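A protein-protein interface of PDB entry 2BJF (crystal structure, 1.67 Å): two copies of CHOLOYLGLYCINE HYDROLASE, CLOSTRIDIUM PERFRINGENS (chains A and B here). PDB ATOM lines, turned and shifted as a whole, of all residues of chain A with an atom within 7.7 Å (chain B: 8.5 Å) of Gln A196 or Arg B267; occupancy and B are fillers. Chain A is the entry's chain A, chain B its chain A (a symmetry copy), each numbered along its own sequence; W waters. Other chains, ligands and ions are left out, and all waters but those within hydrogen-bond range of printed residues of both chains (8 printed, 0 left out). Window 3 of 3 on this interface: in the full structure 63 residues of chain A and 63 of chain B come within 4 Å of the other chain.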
ATOM      1  N   ARG A 193      -6.782   6.750   5.327  1.00  0.00           N
ATOM      2  CA  ARG A 193      -5.507   6.690   6.045  1.00  0.00           C
ATOM      3  C   ARG A 193      -4.719   5.441   5.660  1.00  0.00           C
ATOM      4  O   ARG A 193      -5.271   4.340   5.615  1.00  0.00           O
ATOM      5  CB  ARG A 193      -5.733   6.718   7.561  1.00  0.00           C
ATOM      6  CG  ARG A 193      -6.132   8.082   8.113  1.00  0.00           C
ATOM      7  CD  ARG A 193      -6.381   8.033   9.613  1.00  0.00           C
ATOM      8  NE  ARG A 193      -7.662   7.411   9.946  1.00  0.00           N
ATOM      9  CZ  ARG A 193      -8.149   7.297  11.180  1.00  0.00           C
ATOM     10  NH1 ARG A 193      -7.466   7.758  12.221  1.00  0.00           N
ATOM     11  NH2 ARG A 193      -9.326   6.717  11.376  1.00  0.00           N
ATOM     12  N   TYR A 194      -3.430   5.617   5.383  1.00  0.00           N
ATOM     13  CA  TYR A 194      -2.564   4.490   5.033  1.00  0.00           C
ATOM     14  C   TYR A 194      -2.078   3.772   6.285  1.00  0.00           C
ATOM     15  O   TYR A 194      -1.776   2.577   6.251  1.00  0.00           O
ATOM     16  CB  TYR A 194      -1.369   4.950   4.192  1.00  0.00           C
ATOM     17  CG  TYR A 194      -1.734   5.844   3.028  1.00  0.00           C
ATOM     18  CD1 TYR A 194      -2.724   5.467   2.117  1.00  0.00           C
ATOM     19  CD2 TYR A 194      -1.089   7.064   2.836  1.00  0.00           C
ATOM     20  CE1 TYR A 194      -3.066   6.287   1.049  1.00  0.00           C
ATOM     21  CE2 TYR A 194      -1.423   7.894   1.769  1.00  0.00           C
ATOM     22  CZ  TYR A 194      -2.410   7.495   0.879  1.00  0.00           C
ATOM     23  OH  TYR A 194      -2.746   8.302  -0.180  1.00  0.00           O
ATOM     24  N   ASN A 195      -2.008   4.516   7.386  1.00  0.00           N
ATOM     25  CA  ASN A 195      -1.564   3.979   8.665  1.00  0.00           C
ATOM     26  C   ASN A 195      -2.658   3.176   9.352  1.00  0.00           C
ATOM     27  O   ASN A 195      -3.814   3.600   9.401  1.00  0.00           O
ATOM     28  CB  ASN A 195      -1.083   5.106   9.582  1.00  0.00           C
ATOM     29  CG  ASN A 195       0.160   5.801   9.055  1.00  0.00           C
ATOM     30  OD1 ASN A 195       0.918   5.234   8.267  1.00  0.00           O
ATOM     31  ND2 ASN A 195       0.375   7.038   9.491  1.00  0.00           N
ATOM     32  N   GLN A 196      -2.277   2.016   9.878  1.00  0.00           N
ATOM     33  CA  GLN A 196      -3.198   1.129  10.584  1.00  0.00           C
ATOM     34  C   GLN A 196      -3.907   1.838  11.738  1.00  0.00           C
ATOM     35  O   GLN A 196      -3.281   2.572  12.507  1.00  0.00           O
ATOM     36  CB  GLN A 196      -2.443  -0.103  11.103  1.00  0.00           C
ATOM     37  CG  GLN A 196      -3.283  -1.103  11.905  1.00  0.00           C
ATOM     38  CD  GLN A 196      -4.237  -1.925  11.048  1.00  0.00           C
ATOM     39  OE1 GLN A 196      -4.522  -1.586   9.899  1.00  0.00           O
ATOM     40  NE2 GLN A 196      -4.741  -3.015  11.617  1.00  0.00           N
ATOM     41  N   VAL A 197      -5.220   1.629  11.826  1.00  0.00           N
ATOM     42  CA  VAL A 197      -6.001   2.052  12.985  1.00  0.00           C
ATOM     43  C   VAL A 197      -6.257   0.796  13.828  1.00  0.00           C
ATOM     44  O   VAL A 197      -7.112  -0.022  13.481  1.00  0.00           O
ATOM     45  CB  VAL A 197      -7.333   2.739  12.579  1.00  0.00           C
ATOM     46  CG1 VAL A 197      -8.073   3.252  13.810  1.00  0.00           C
ATOM     47  CG2 VAL A 197      -7.071   3.887  11.612  1.00  0.00           C
ATOM     48  N   PRO A 198      -5.487   0.624  14.921  1.00  0.00           N
ATOM     49  CA  PRO A 198      -5.498  -0.627  15.684  1.00  0.00           C
ATOM     50  C   PRO A 198      -6.717  -0.834  16.586  1.00  0.00           C
ATOM     51  O   PRO A 198      -7.076  -1.979  16.874  1.00  0.00           O
ATOM     52  CB  PRO A 198      -4.226  -0.527  16.532  1.00  0.00           C
ATOM     53  CG  PRO A 198      -4.018   0.929  16.723  1.00  0.00           C
ATOM     54  CD  PRO A 198      -4.542   1.608  15.487  1.00  0.00           C
ATOM     55  N   GLU A 199      -7.335   0.257  17.035  1.00  0.00           N
ATOM     56  CA  GLU A 199      -8.458   0.165  17.967  1.00  0.00           C
ATOM     57  C   GLU A 199      -9.424   1.343  17.897  1.00  0.00           C
ATOM     58  O   GLU A 199      -9.100   2.401  17.353  1.00  0.00           O
ATOM     59  CB  GLU A 199      -7.960  -0.029  19.409  1.00  0.00           C
ATOM     60  CG  GLU A 199      -7.080   1.098  19.946  1.00  0.00           C
ATOM     61  CD  GLU A 199      -6.669   0.894  21.397  1.00  0.00           C
ATOM     62  OE1 GLU A 199      -6.787  -0.241  21.910  1.00  0.00           O
ATOM     63  OE2 GLU A 199      -6.222   1.875  22.028  1.00  0.00           O
ATOM     64  N   THR A 208     -11.337  -3.838  18.145  1.00  0.00           N
ATOM     65  CA  THR A 208      -9.954  -4.119  17.769  1.00  0.00           C
ATOM     66  C   THR A 208      -9.844  -4.457  16.284  1.00  0.00           C
ATOM     67  O   THR A 208     -10.669  -5.199  15.745  1.00  0.00           O
ATOM     68  CB  THR A 208      -9.332  -5.246  18.649  1.00  0.00           C
ATOM     69  OG1 THR A 208      -7.989  -5.515  18.228  1.00  0.00           O
ATOM     70  CG2 THR A 208     -10.153  -6.531  18.579  1.00  0.00           C
ATOM     71  N   ALA A 209      -8.832  -3.894  15.629  1.00  0.00           N
ATOM     72  CA  ALA A 209      -8.551  -4.203  14.231  1.00  0.00           C
ATOM     73  C   ALA A 209      -8.311  -5.700  14.089  1.00  0.00           C
ATOM     74  O   ALA A 209      -7.542  -6.284  14.853  1.00  0.00           O
ATOM     75  CB  ALA A 209      -7.345  -3.422  13.748  1.00  0.00           C
ATOM     76  N   LEU A 210      -8.986  -6.319  13.126  1.00  0.00           N
ATOM     77  CA  LEU A 210      -8.886  -7.767  12.944  1.00  0.00           C
ATOM     78  C   LEU A 210      -7.803  -8.157  11.947  1.00  0.00           C
ATOM     79  O   LEU A 210      -7.426  -9.324  11.853  1.00  0.00           O
ATOM     80  CB  LEU A 210     -10.242  -8.367  12.558  1.00  0.00           C
ATOM     81  CG  LEU A 210     -11.388  -8.154  13.560  1.00  0.00           C
ATOM     82  CD1 LEU A 210     -12.632  -8.876  13.110  1.00  0.00           C
ATOM     83  CD2 LEU A 210     -11.018  -8.584  14.975  1.00  0.00           C
ATOM     84  N   GLY A 211      -7.305  -7.165  11.215  1.00  0.00           N
ATOM     85  CA  GLY A 211      -6.203  -7.349  10.281  1.00  0.00           C
ATOM     86  C   GLY A 211      -5.677  -6.009   9.807  1.00  0.00           C
ATOM     87  O   GLY A 211      -6.225  -4.960  10.158  1.00  0.00           O
ATOM     88  N   GLN A 212      -4.616  -6.043   9.008  1.00  0.00           N
ATOM     89  CA  GLN A 212      -4.036  -4.823   8.457  1.00  0.00           C
ATOM     90  C   GLN A 212      -4.942  -4.196   7.403  1.00  0.00           C
ATOM     91  O   GLN A 212      -5.608  -4.907   6.646  1.00  0.00           O
ATOM     92  CB  GLN A 212      -2.653  -5.103   7.854  1.00  0.00           C
ATOM     93  CG  GLN A 212      -1.563  -5.430   8.872  1.00  0.00           C
ATOM     94  CD  GLN A 212      -1.322  -4.317   9.888  1.00  0.00           C
ATOM     95  OE1 GLN A 212      -1.117  -4.585  11.069  1.00  0.00           O
ATOM     96  NE2 GLN A 212      -1.339  -3.069   9.431  1.00  0.00           N
ATOM     97  N   GLY A 213      -4.970  -2.866   7.374  1.00  0.00           N
ATOM     98  CA  GLY A 213      -5.674  -2.120   6.331  1.00  0.00           C
ATOM     99  C   GLY A 213      -6.927  -1.371   6.753  1.00  0.00           C
ATOM    100  O   GLY A 213      -7.690  -0.912   5.904  1.00  0.00           O
ATOM    101  N   THR A 214      -7.138  -1.229   8.059  1.00  0.00           N
ATOM    102  CA  THR A 214      -8.370  -0.617   8.573  1.00  0.00           C
ATOM    103  C   THR A 214      -8.522   0.867   8.239  1.00  0.00           C
ATOM    104  O   THR A 214      -9.636   1.396   8.234  1.00  0.00           O
ATOM    105  CB  THR A 214      -8.517  -0.813  10.094  1.00  0.00           C
ATOM    106  OG1 THR A 214      -7.354  -0.307  10.760  1.00  0.00           O
ATOM    107  CG2 THR A 214      -8.705  -2.289  10.430  1.00  0.00           C
ATOM    108  N   GLY A 215      -7.407   1.532   7.945  1.00  0.00           N
ATOM    109  CA  GLY A 215      -7.425   2.955   7.614  1.00  0.00           C
ATOM    110  C   GLY A 215      -8.048   3.279   6.265  1.00  0.00           C
ATOM    111  O   GLY A 215      -8.529   4.395   6.054  1.00  0.00           O
ATOM    112  N   LEU A 216      -8.035   2.308   5.352  1.00  0.00           N
ATOM    113  CA  LEU A 216      -8.548   2.513   3.992  1.00  0.00           C
ATOM    114  C   LEU A 216      -9.962   1.980   3.759  1.00  0.00           C
ATOM    115  O   LEU A 216     -10.460   2.012   2.630  1.00  0.00           O
ATOM    116  CB  LEU A 216      -7.591   1.919   2.950  1.00  0.00           C
ATOM    117  CG  LEU A 216      -6.249   2.602   2.683  1.00  0.00           C
ATOM    118  CD1 LEU A 216      -5.562   1.924   1.507  1.00  0.00           C
ATOM    119  CD2 LEU A 216      -6.417   4.094   2.408  1.00  0.00           C
ATOM    120  N   ALA A 238       0.460   7.062  -1.691  1.00  0.00           N
ATOM    121  CA  ALA A 238       1.004   6.345  -0.541  1.00  0.00           C
ATOM    122  C   ALA A 238       2.438   5.889  -0.772  1.00  0.00           C
ATOM    123  O   ALA A 238       3.275   5.970   0.130  1.00  0.00           O
ATOM    124  CB  ALA A 238       0.127   5.159  -0.197  1.00  0.00           C
ATOM    125  N   LYS A 241       4.766   9.017  -0.741  1.00  0.00           N
ATOM    126  CA  LYS A 241       4.881   9.514   0.629  1.00  0.00           C
ATOM    127  C   LYS A 241       5.788   8.656   1.507  1.00  0.00           C
ATOM    128  O   LYS A 241       6.661   9.179   2.203  1.00  0.00           O
ATOM    129  CB  LYS A 241       3.501   9.618   1.278  1.00  0.00           C
ATOM    130  CG  LYS A 241       2.750  10.875   0.925  1.00  0.00           C
ATOM    131  CD  LYS A 241       1.357  10.833   1.505  1.00  0.00           C
ATOM    132  CE  LYS A 241       0.668  12.166   1.348  1.00  0.00           C
ATOM    133  NZ  LYS A 241      -0.786  12.036   1.587  1.00  0.00           N
ATOM    134  N   ASN A 242       5.581   7.343   1.462  1.00  0.00           N
ATOM    135  CA  ASN A 242       6.235   6.429   2.395  1.00  0.00           C
ATOM    136  C   ASN A 242       7.451   5.680   1.851  1.00  0.00           C
ATOM    137  O   ASN A 242       8.285   5.211   2.629  1.00  0.00           O
ATOM    138  CB  ASN A 242       5.215   5.436   2.962  1.00  0.00           C
ATOM    139  CG  ASN A 242       4.156   6.111   3.815  1.00  0.00           C
ATOM    140  OD1 ASN A 242       4.462   6.970   4.645  1.00  0.00           O
ATOM    141  ND2 ASN A 242       2.902   5.722   3.617  1.00  0.00           N
ATOM    142  N   ASP A 243       7.553   5.571   0.528  1.00  0.00           N
ATOM    143  CA  ASP A 243       8.579   4.729  -0.094  1.00  0.00           C
ATOM    144  C   ASP A 243       9.161   5.316  -1.384  1.00  0.00           C
ATOM    145  O   ASP A 243       9.434   4.585  -2.341  1.00  0.00           O
ATOM    146  CB  ASP A 243       8.015   3.325  -0.350  1.00  0.00           C
ATOM    147  CG  ASP A 243       7.727   2.568   0.933  1.00  0.00           C
ATOM    148  OD1 ASP A 243       8.686   2.074   1.565  1.00  0.00           O
ATOM    149  OD2 ASP A 243       6.540   2.465   1.312  1.00  0.00           O
ATOM    150  N   GLU B  23       5.237  -8.034   6.305  1.00  0.00           N
ATOM    151  CA  GLU B  23       6.111  -6.863   6.197  1.00  0.00           C
ATOM    152  C   GLU B  23       7.591  -7.209   6.407  1.00  0.00           C
ATOM    153  O   GLU B  23       8.443  -6.319   6.510  1.00  0.00           O
ATOM    154  CB  GLU B  23       5.657  -5.759   7.170  1.00  0.00           C
ATOM    155  CG  GLU B  23       5.964  -6.013   8.655  1.00  0.00           C
ATOM    156  CD  GLU B  23       4.899  -6.829   9.382  1.00  0.00           C
ATOM    157  OE1 GLU B  23       4.325  -7.768   8.790  1.00  0.00           O
ATOM    158  OE2 GLU B  23       4.648  -6.533  10.570  1.00  0.00           O
ATOM    159  N   PHE B 223      -7.833  -3.370   1.910  1.00  0.00           N
ATOM    160  CA  PHE B 223      -6.975  -4.548   2.030  1.00  0.00           C
ATOM    161  C   PHE B 223      -7.170  -5.335   3.328  1.00  0.00           C
ATOM    162  O   PHE B 223      -6.346  -6.193   3.660  1.00  0.00           O
ATOM    163  CB  PHE B 223      -5.503  -4.152   1.841  1.00  0.00           C
ATOM    164  CG  PHE B 223      -5.212  -3.521   0.507  1.00  0.00           C
ATOM    165  CD1 PHE B 223      -4.934  -4.312  -0.604  1.00  0.00           C
ATOM    166  CD2 PHE B 223      -5.221  -2.136   0.360  1.00  0.00           C
ATOM    167  CE1 PHE B 223      -4.672  -3.733  -1.845  1.00  0.00           C
ATOM    168  CE2 PHE B 223      -4.958  -1.547  -0.878  1.00  0.00           C
ATOM    169  CZ  PHE B 223      -4.680  -2.348  -1.979  1.00  0.00           C
ATOM    170  N   THR B 224      -8.258  -5.064   4.053  1.00  0.00           N
ATOM    171  CA  THR B 224      -8.580  -5.862   5.243  1.00  0.00           C
ATOM    172  C   THR B 224      -8.919  -7.296   4.836  1.00  0.00           C
ATOM    173  O   THR B 224      -9.345  -7.535   3.700  1.00  0.00           O
ATOM    174  CB  THR B 224      -9.754  -5.285   6.073  1.00  0.00           C
ATOM    175  OG1 THR B 224     -10.943  -5.249   5.274  1.00  0.00           O
ATOM    176  CG2 THR B 224      -9.423  -3.898   6.608  1.00  0.00           C
ATOM    177  N   PRO B 225      -8.717  -8.260   5.753  1.00  0.00           N
ATOM    178  CA  PRO B 225      -9.046  -9.658   5.459  1.00  0.00           C
ATOM    179  C   PRO B 225     -10.488  -9.874   4.987  1.00  0.00           C
ATOM    180  O   PRO B 225     -10.707 -10.633   4.042  1.00  0.00           O
ATOM    181  CB  PRO B 225      -8.794 -10.365   6.792  1.00  0.00           C
ATOM    182  CG  PRO B 225      -7.785  -9.513   7.482  1.00  0.00           C
ATOM    183  CD  PRO B 225      -8.138  -8.106   7.102  1.00  0.00           C
ATOM    184  N   MET B 261      -1.278  -6.742  -1.725  1.00  0.00           N
ATOM    185  CA  MET B 261      -0.903  -5.487  -1.075  1.00  0.00           C
ATOM    186  C   MET B 261       0.232  -4.797  -1.826  1.00  0.00           C
ATOM    187  O   MET B 261       1.144  -5.458  -2.336  1.00  0.00           O
ATOM    188  CB  MET B 261      -0.509  -5.721   0.383  1.00  0.00           C
ATOM    189  CG  MET B 261      -1.657  -6.173   1.265  1.00  0.00           C
ATOM    190  SD  MET B 261      -1.122  -6.548   2.939  1.00  0.00           S
ATOM    191  CE  MET B 261      -2.621  -7.262   3.605  1.00  0.00           C
ATOM    192  N   VAL B 262       0.161  -3.469  -1.876  1.00  0.00           N
ATOM    193  CA  VAL B 262       1.085  -2.633  -2.647  1.00  0.00           C
ATOM    194  C   VAL B 262       1.885  -1.739  -1.698  1.00  0.00           C
ATOM    195  O   VAL B 262       1.320  -1.150  -0.773  1.00  0.00           O
ATOM    196  CB  VAL B 262       0.312  -1.753  -3.671  1.00  0.00           C
ATOM    197  CG1 VAL B 262       1.268  -0.948  -4.541  1.00  0.00           C
ATOM    198  CG2 VAL B 262      -0.602  -2.610  -4.545  1.00  0.00           C
ATOM    199  N   ARG B 263       3.195  -1.642  -1.931  1.00  0.00           N
ATOM    200  CA  ARG B 263       4.095  -0.875  -1.062  1.00  0.00           C
ATOM    201  C   ARG B 263       3.600   0.541  -0.776  1.00  0.00           C
ATOM    202  O   ARG B 263       3.277   1.293  -1.699  1.00  0.00           O
ATOM    203  CB  ARG B 263       5.512  -0.821  -1.649  1.00  0.00           C
ATOM    204  CG  ARG B 263       6.585  -0.436  -0.636  1.00  0.00           C
ATOM    205  CD  ARG B 263       7.962  -0.282  -1.277  1.00  0.00           C
ATOM    206  NE  ARG B 263       8.456  -1.525  -1.867  1.00  0.00           N
ATOM    207  CZ  ARG B 263       9.120  -2.472  -1.209  1.00  0.00           C
ATOM    208  NH1 ARG B 263       9.385  -2.343   0.087  1.00  0.00           N
ATOM    209  NH2 ARG B 263       9.520  -3.559  -1.856  1.00  0.00           N
ATOM    210  N   GLY B 264       3.539   0.884   0.509  1.00  0.00           N
ATOM    211  CA  GLY B 264       3.213   2.239   0.942  1.00  0.00           C
ATOM    212  C   GLY B 264       1.817   2.464   1.498  1.00  0.00           C
ATOM    213  O   GLY B 264       1.622   3.344   2.338  1.00  0.00           O
ATOM    214  N   SER B 265       0.845   1.678   1.035  1.00  0.00           N
ATOM    215  CA  SER B 265      -0.570   1.931   1.346  1.00  0.00           C
ATOM    216  C   SER B 265      -1.165   1.095   2.477  1.00  0.00           C
ATOM    217  O   SER B 265      -2.238   1.423   2.992  1.00  0.00           O
ATOM    218  CB  SER B 265      -1.435   1.814   0.085  1.00  0.00           C
ATOM    219  OG  SER B 265      -1.111   0.655  -0.661  1.00  0.00           O
ATOM    220  N   THR B 266      -0.482   0.016   2.851  1.00  0.00           N
ATOM    221  CA  THR B 266      -0.869  -0.782   4.015  1.00  0.00           C
ATOM    222  C   THR B 266       0.252  -0.717   5.052  1.00  0.00           C
ATOM    223  O   THR B 266       1.123  -1.590   5.109  1.00  0.00           O
ATOM    224  CB  THR B 266      -1.212  -2.246   3.629  1.00  0.00           C
ATOM    225  OG1 THR B 266      -2.198  -2.247   2.590  1.00  0.00           O
ATOM    226  CG2 THR B 266      -1.760  -3.021   4.831  1.00  0.00           C
ATOM    227  N   ARG B 267       0.221   0.340   5.858  1.00  0.00           N
ATOM    228  CA  ARG B 267       1.269   0.607   6.842  1.00  0.00           C
ATOM    229  C   ARG B 267       0.897   0.070   8.217  1.00  0.00           C
ATOM    230  O   ARG B 267      -0.178   0.370   8.741  1.00  0.00           O
ATOM    231  CB  ARG B 267       1.554   2.112   6.927  1.00  0.00           C
ATOM    232  CG  ARG B 267       1.954   2.764   5.603  1.00  0.00           C
ATOM    233  CD  ARG B 267       3.416   2.515   5.254  1.00  0.00           C
ATOM    234  NE  ARG B 267       4.313   3.369   6.031  1.00  0.00           N
ATOM    235  CZ  ARG B 267       5.641   3.363   5.929  1.00  0.00           C
ATOM    236  NH1 ARG B 267       6.248   2.542   5.083  1.00  0.00           N
ATOM    237  NH2 ARG B 267       6.364   4.183   6.680  1.00  0.00           N
ATOM    238  N   THR B 268       1.795  -0.724   8.796  1.00  0.00           N
ATOM    239  CA  THR B 268       1.611  -1.259  10.146  1.00  0.00           C
ATOM    240  C   THR B 268       1.838  -0.158  11.182  1.00  0.00           C
ATOM    241  O   THR B 268       2.330   0.923  10.848  1.00  0.00           O
ATOM    242  CB  THR B 268       2.578  -2.430  10.427  1.00  0.00           C
ATOM    243  OG1 THR B 268       3.928  -1.950  10.435  1.00  0.00           O
ATOM    244  CG2 THR B 268       2.431  -3.529   9.373  1.00  0.00           C
ATOM    245  N   VAL B 269       1.483  -0.434  12.438  1.00  0.00           N
ATOM    246  CA  VAL B 269       1.704   0.526  13.529  1.00  0.00           C
ATOM    247  C   VAL B 269       3.196   0.779  13.787  1.00  0.00           C
ATOM    248  O   VAL B 269       3.565   1.801  14.368  1.00  0.00           O
ATOM    249  CB  VAL B 269       0.978   0.118  14.847  1.00  0.00           C
ATOM    250  CG1 VAL B 269      -0.535   0.121  14.652  1.00  0.00           C
ATOM    251  CG2 VAL B 269       1.462  -1.237  15.363  1.00  0.00           C
ATOM    252  N   GLU B 270       4.039  -0.149  13.334  1.00  0.00           N
ATOM    253  CA  GLU B 270       5.494  -0.004  13.422  1.00  0.00           C
ATOM    254  C   GLU B 270       6.063   0.754  12.217  1.00  0.00           C
ATOM    255  O   GLU B 270       7.284   0.852  12.053  1.00  0.00           O
ATOM    256  CB  GLU B 270       6.173  -1.371  13.559  1.00  0.00           C
ATOM    257  CG  GLU B 270       5.894  -2.101  14.874  1.00  0.00           C
ATOM    258  CD  GLU B 270       4.605  -2.907  14.855  1.00  0.00           C
ATOM    259  OE1 GLU B 270       4.062  -3.160  13.758  1.00  0.00           O
ATOM    260  OE2 GLU B 270       4.135  -3.293  15.947  1.00  0.00           O
ATOM    261  N   GLU B 271       5.166   1.286  11.384  1.00  0.00           N
ATOM    262  CA  GLU B 271       5.515   2.094  10.208  1.00  0.00           C
ATOM    263  C   GLU B 271       6.338   1.321   9.169  1.00  0.00           C
ATOM    264  O   GLU B 271       7.349   1.809   8.657  1.00  0.00           O
ATOM    265  CB  GLU B 271       6.190   3.413  10.619  1.00  0.00           C
ATOM    266  CG  GLU B 271       5.254   4.376  11.349  1.00  0.00           C
ATOM    267  CD  GLU B 271       5.967   5.576  11.953  1.00  0.00           C
ATOM    268  OE1 GLU B 271       6.959   6.058  11.365  1.00  0.00           O
ATOM    269  OE2 GLU B 271       5.521   6.046  13.022  1.00  0.00           O
ATOM    270  N   LYS B 272       5.882   0.105   8.875  1.00  0.00           N
ATOM    271  CA  LYS B 272       6.448  -0.718   7.810  1.00  0.00           C
ATOM    272  C   LYS B 272       5.363  -1.040   6.790  1.00  0.00           C
ATOM    273  O   LYS B 272       4.189  -1.173   7.145  1.00  0.00           O
ATOM    274  CB  LYS B 272       7.024  -2.018   8.377  1.00  0.00           C
ATOM    275  CG  LYS B 272       8.372  -1.868   9.076  1.00  0.00           C
ATOM    276  CD  LYS B 272       8.804  -3.169   9.747  1.00  0.00           C
ATOM    277  CE  LYS B 272       8.199  -3.299  11.140  1.00  0.00           C
ATOM    278  NZ  LYS B 272       8.415  -4.636  11.759  1.00  0.00           N
ATOM    279  N   SER B 273       5.758  -1.162   5.526  1.00  0.00           N
ATOM    280  CA  SER B 273       4.820  -1.506   4.463  1.00  0.00           C
ATOM    281  C   SER B 273       4.554  -3.006   4.404  1.00  0.00           C
ATOM    282  O   SER B 273       5.473  -3.809   4.209  1.00  0.00           O
ATOM    283  CB  SER B 273       5.314  -0.996   3.106  1.00  0.00           C
ATOM    284  OG  SER B 273       5.238   0.415   3.040  1.00  0.00           O
ATOM    285  N   ASP B 274       3.290  -3.371   4.592  1.00  0.00           N
ATOM    286  CA  ASP B 274       2.833  -4.744   4.424  1.00  0.00           C
ATOM    287  C   ASP B 274       2.704  -5.013   2.926  1.00  0.00           C
ATOM    288  O   ASP B 274       2.053  -4.248   2.208  1.00  0.00           O
ATOM    289  CB  ASP B 274       1.485  -4.932   5.129  1.00  0.00           C
ATOM    290  CG  ASP B 274       1.205  -6.377   5.511  1.00  0.00           C
ATOM    291  OD1 ASP B 274       2.007  -7.274   5.178  1.00  0.00           O
ATOM    292  OD2 ASP B 274       0.160  -6.616   6.155  1.00  0.00           O
ATOM    293  N   LEU B 275       3.343  -6.084   2.459  1.00  0.00           N
ATOM    294  CA  LEU B 275       3.386  -6.410   1.031  1.00  0.00           C
ATOM    295  C   LEU B 275       2.936  -7.837   0.768  1.00  0.00           C
ATOM    296  O   LEU B 275       3.090  -8.705   1.626  1.00  0.00           O
ATOM    297  CB  LEU B 275       4.817  -6.275   0.483  1.00  0.00           C
ATOM    298  CG  LEU B 275       5.740  -5.110   0.845  1.00  0.00           C
ATOM    299  CD1 LEU B 275       7.092  -5.278   0.164  1.00  0.00           C
ATOM    300  CD2 LEU B 275       5.119  -3.786   0.466  1.00  0.00           C
HETATM  301  O   HOH W   1       1.401   3.459  11.204  1.00  0.00           O
HETATM  302  O   HOH W   2       3.540   4.815   8.317  1.00  0.00           O
HETATM  303  O   HOH W   3      -6.823  -1.294   3.393  1.00  0.00           O
HETATM  304  O   HOH W   4      -2.465  -0.743   7.629  1.00  0.00           O
HETATM  305  O   HOH W   5      -4.934  -7.627   6.016  1.00  0.00           O
HETATM  306  O   HOH W   6       8.871  -0.731   2.425  1.00  0.00           O
HETATM  307  O   HOH W   7       8.968   2.348   4.499  1.00  0.00           O
HETATM  308  O   HOH W   8       0.058  -2.980  12.896  1.00  0.00           O
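Tyr A194 touches Gly B264 (CB to O, 3.9 Å). Arg B267 touches Asn A195 (CB to OD1, 3.5 Å). Pro B225 touches Gly A211 (CD to CA, 3.8 Å). O of Gln A212 touches CA of Thr B224 (3.4 Å). CB of Gln A212 touches CG2 of Thr B266, at 3.8 Å. Thr B268 touches Gln A212. Thr B224 touches Gly A213. Ala A238 touches Ser B265. Asn A242 touches Arg B267. Asp A243 touches Arg B263.
No position is printed for both chains.
O of Gly A211 is in hydrogen-bond range of NE2 of Gln A196 (2.8 Å). The backbone NH (N) of Thr A214 sits at hydrogen-bond distance from the side-chain amide oxygen (OE1) of Gln A196, at 3.2 Å. The side-chain hydroxyl (OG) of Ser B273 sits at hydrogen-bond distance from the backbone NH (N) of Gly B264 (3.1 Å). O of Thr B266 lies within hydrogen-bond range of N of Asp B274. The backbone NH (N) of Lys B272 lies within hydrogen-bond range of the side-chain hydroxyl (OG1) of Thr B268 (3.2 Å).
Water W2 bridges OD1 of Asn A195 and NE of Arg B267. Water W3 bridges the backbone carbonyl oxygen of Gly A213 (2.7 Å) and the backbone NH of Phe B223 (2.7 Å). Water W4 lies within hydrogen-bond range of the backbone carbonyl oxygen (O) of Arg B267 (2.8 Å), the side-chain amide nitrogen (NE2) of Gln A212 (3.2 Å), the side-chain amide oxygen (OE1) of Gln A196 (3.2 Å) and the backbone NH (N) of Gly A213 (3.3 Å).
Hydrophobic or aromatic side chains of chain A within 4 Å of the printed part of chain B: Tyr A194, Leu A216 and Ala A238. Hydrophobic or aromatic side chains of chain B that line the printed part of chain A: Pro B225. Among the printed residues, 23 pairs touch across the chains. Among the printed residues, Asp or Glu carboxylates within 4 Å of a Lys or Arg side-chain nitrogen of the other chain: Asp A243 with Arg B267.
Gln A196 touches just one residue of chain B: Arg B267 (2.9 Å). Arg B267 touches just these residues of chain A: Tyr A194 (3.0 Å), Asn A195 (3.5 Å), Gln A196 (2.9 Å), Gln A212 (3.7 Å), Asn A242 (3.5 Å) and Asp A243 (3.8 Å). Printed residues of chain A within 4 Å of Phe B223: Gln A212. Printed residues of chain B within 4 Å of Gly A213: Thr B224. Thr A208 touches none of the printed residues of chain B. Gly A215 touches none of the printed residues of chain B. The nearest residue of chain B that does not touch Gln A196 is Val B269 (4.04 Å). The nearest printed residue of chain B that does not touch Gln A212 is Pro B225 (4.1 Å).
O of Tyr A194 lies within hydrogen-bond range of N of Arg B267 (3.0 Å). The backbone carbonyl oxygen (O) of Arg B267 is in hydrogen-bond range of the backbone NH (N) of Gln A196 (2.9 Å). ND2 of Asn A242 sits at hydrogen-bond distance from O of Gly B264. The backbone NH (N) of Gly B264 lies close to the side-chain carboxylate (OD2) of Asp A243. The side-chain carboxylate (OD2) of Asp A243 lies within salt-bridge range of the guanidinium group (NH1) of Arg B267 (3.8 Å). OG of Ser B273 is in hydrogen-bond range of OD2 of Asp A243 (3.0 Å). The backbone carbonyl oxygen (O) of Ser B265 sits close to the backbone carbonyl oxygen (O) of Tyr A194, at 3.5 Å. O of Gln A212 sits close to O of Phe B223 (3.3 Å).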
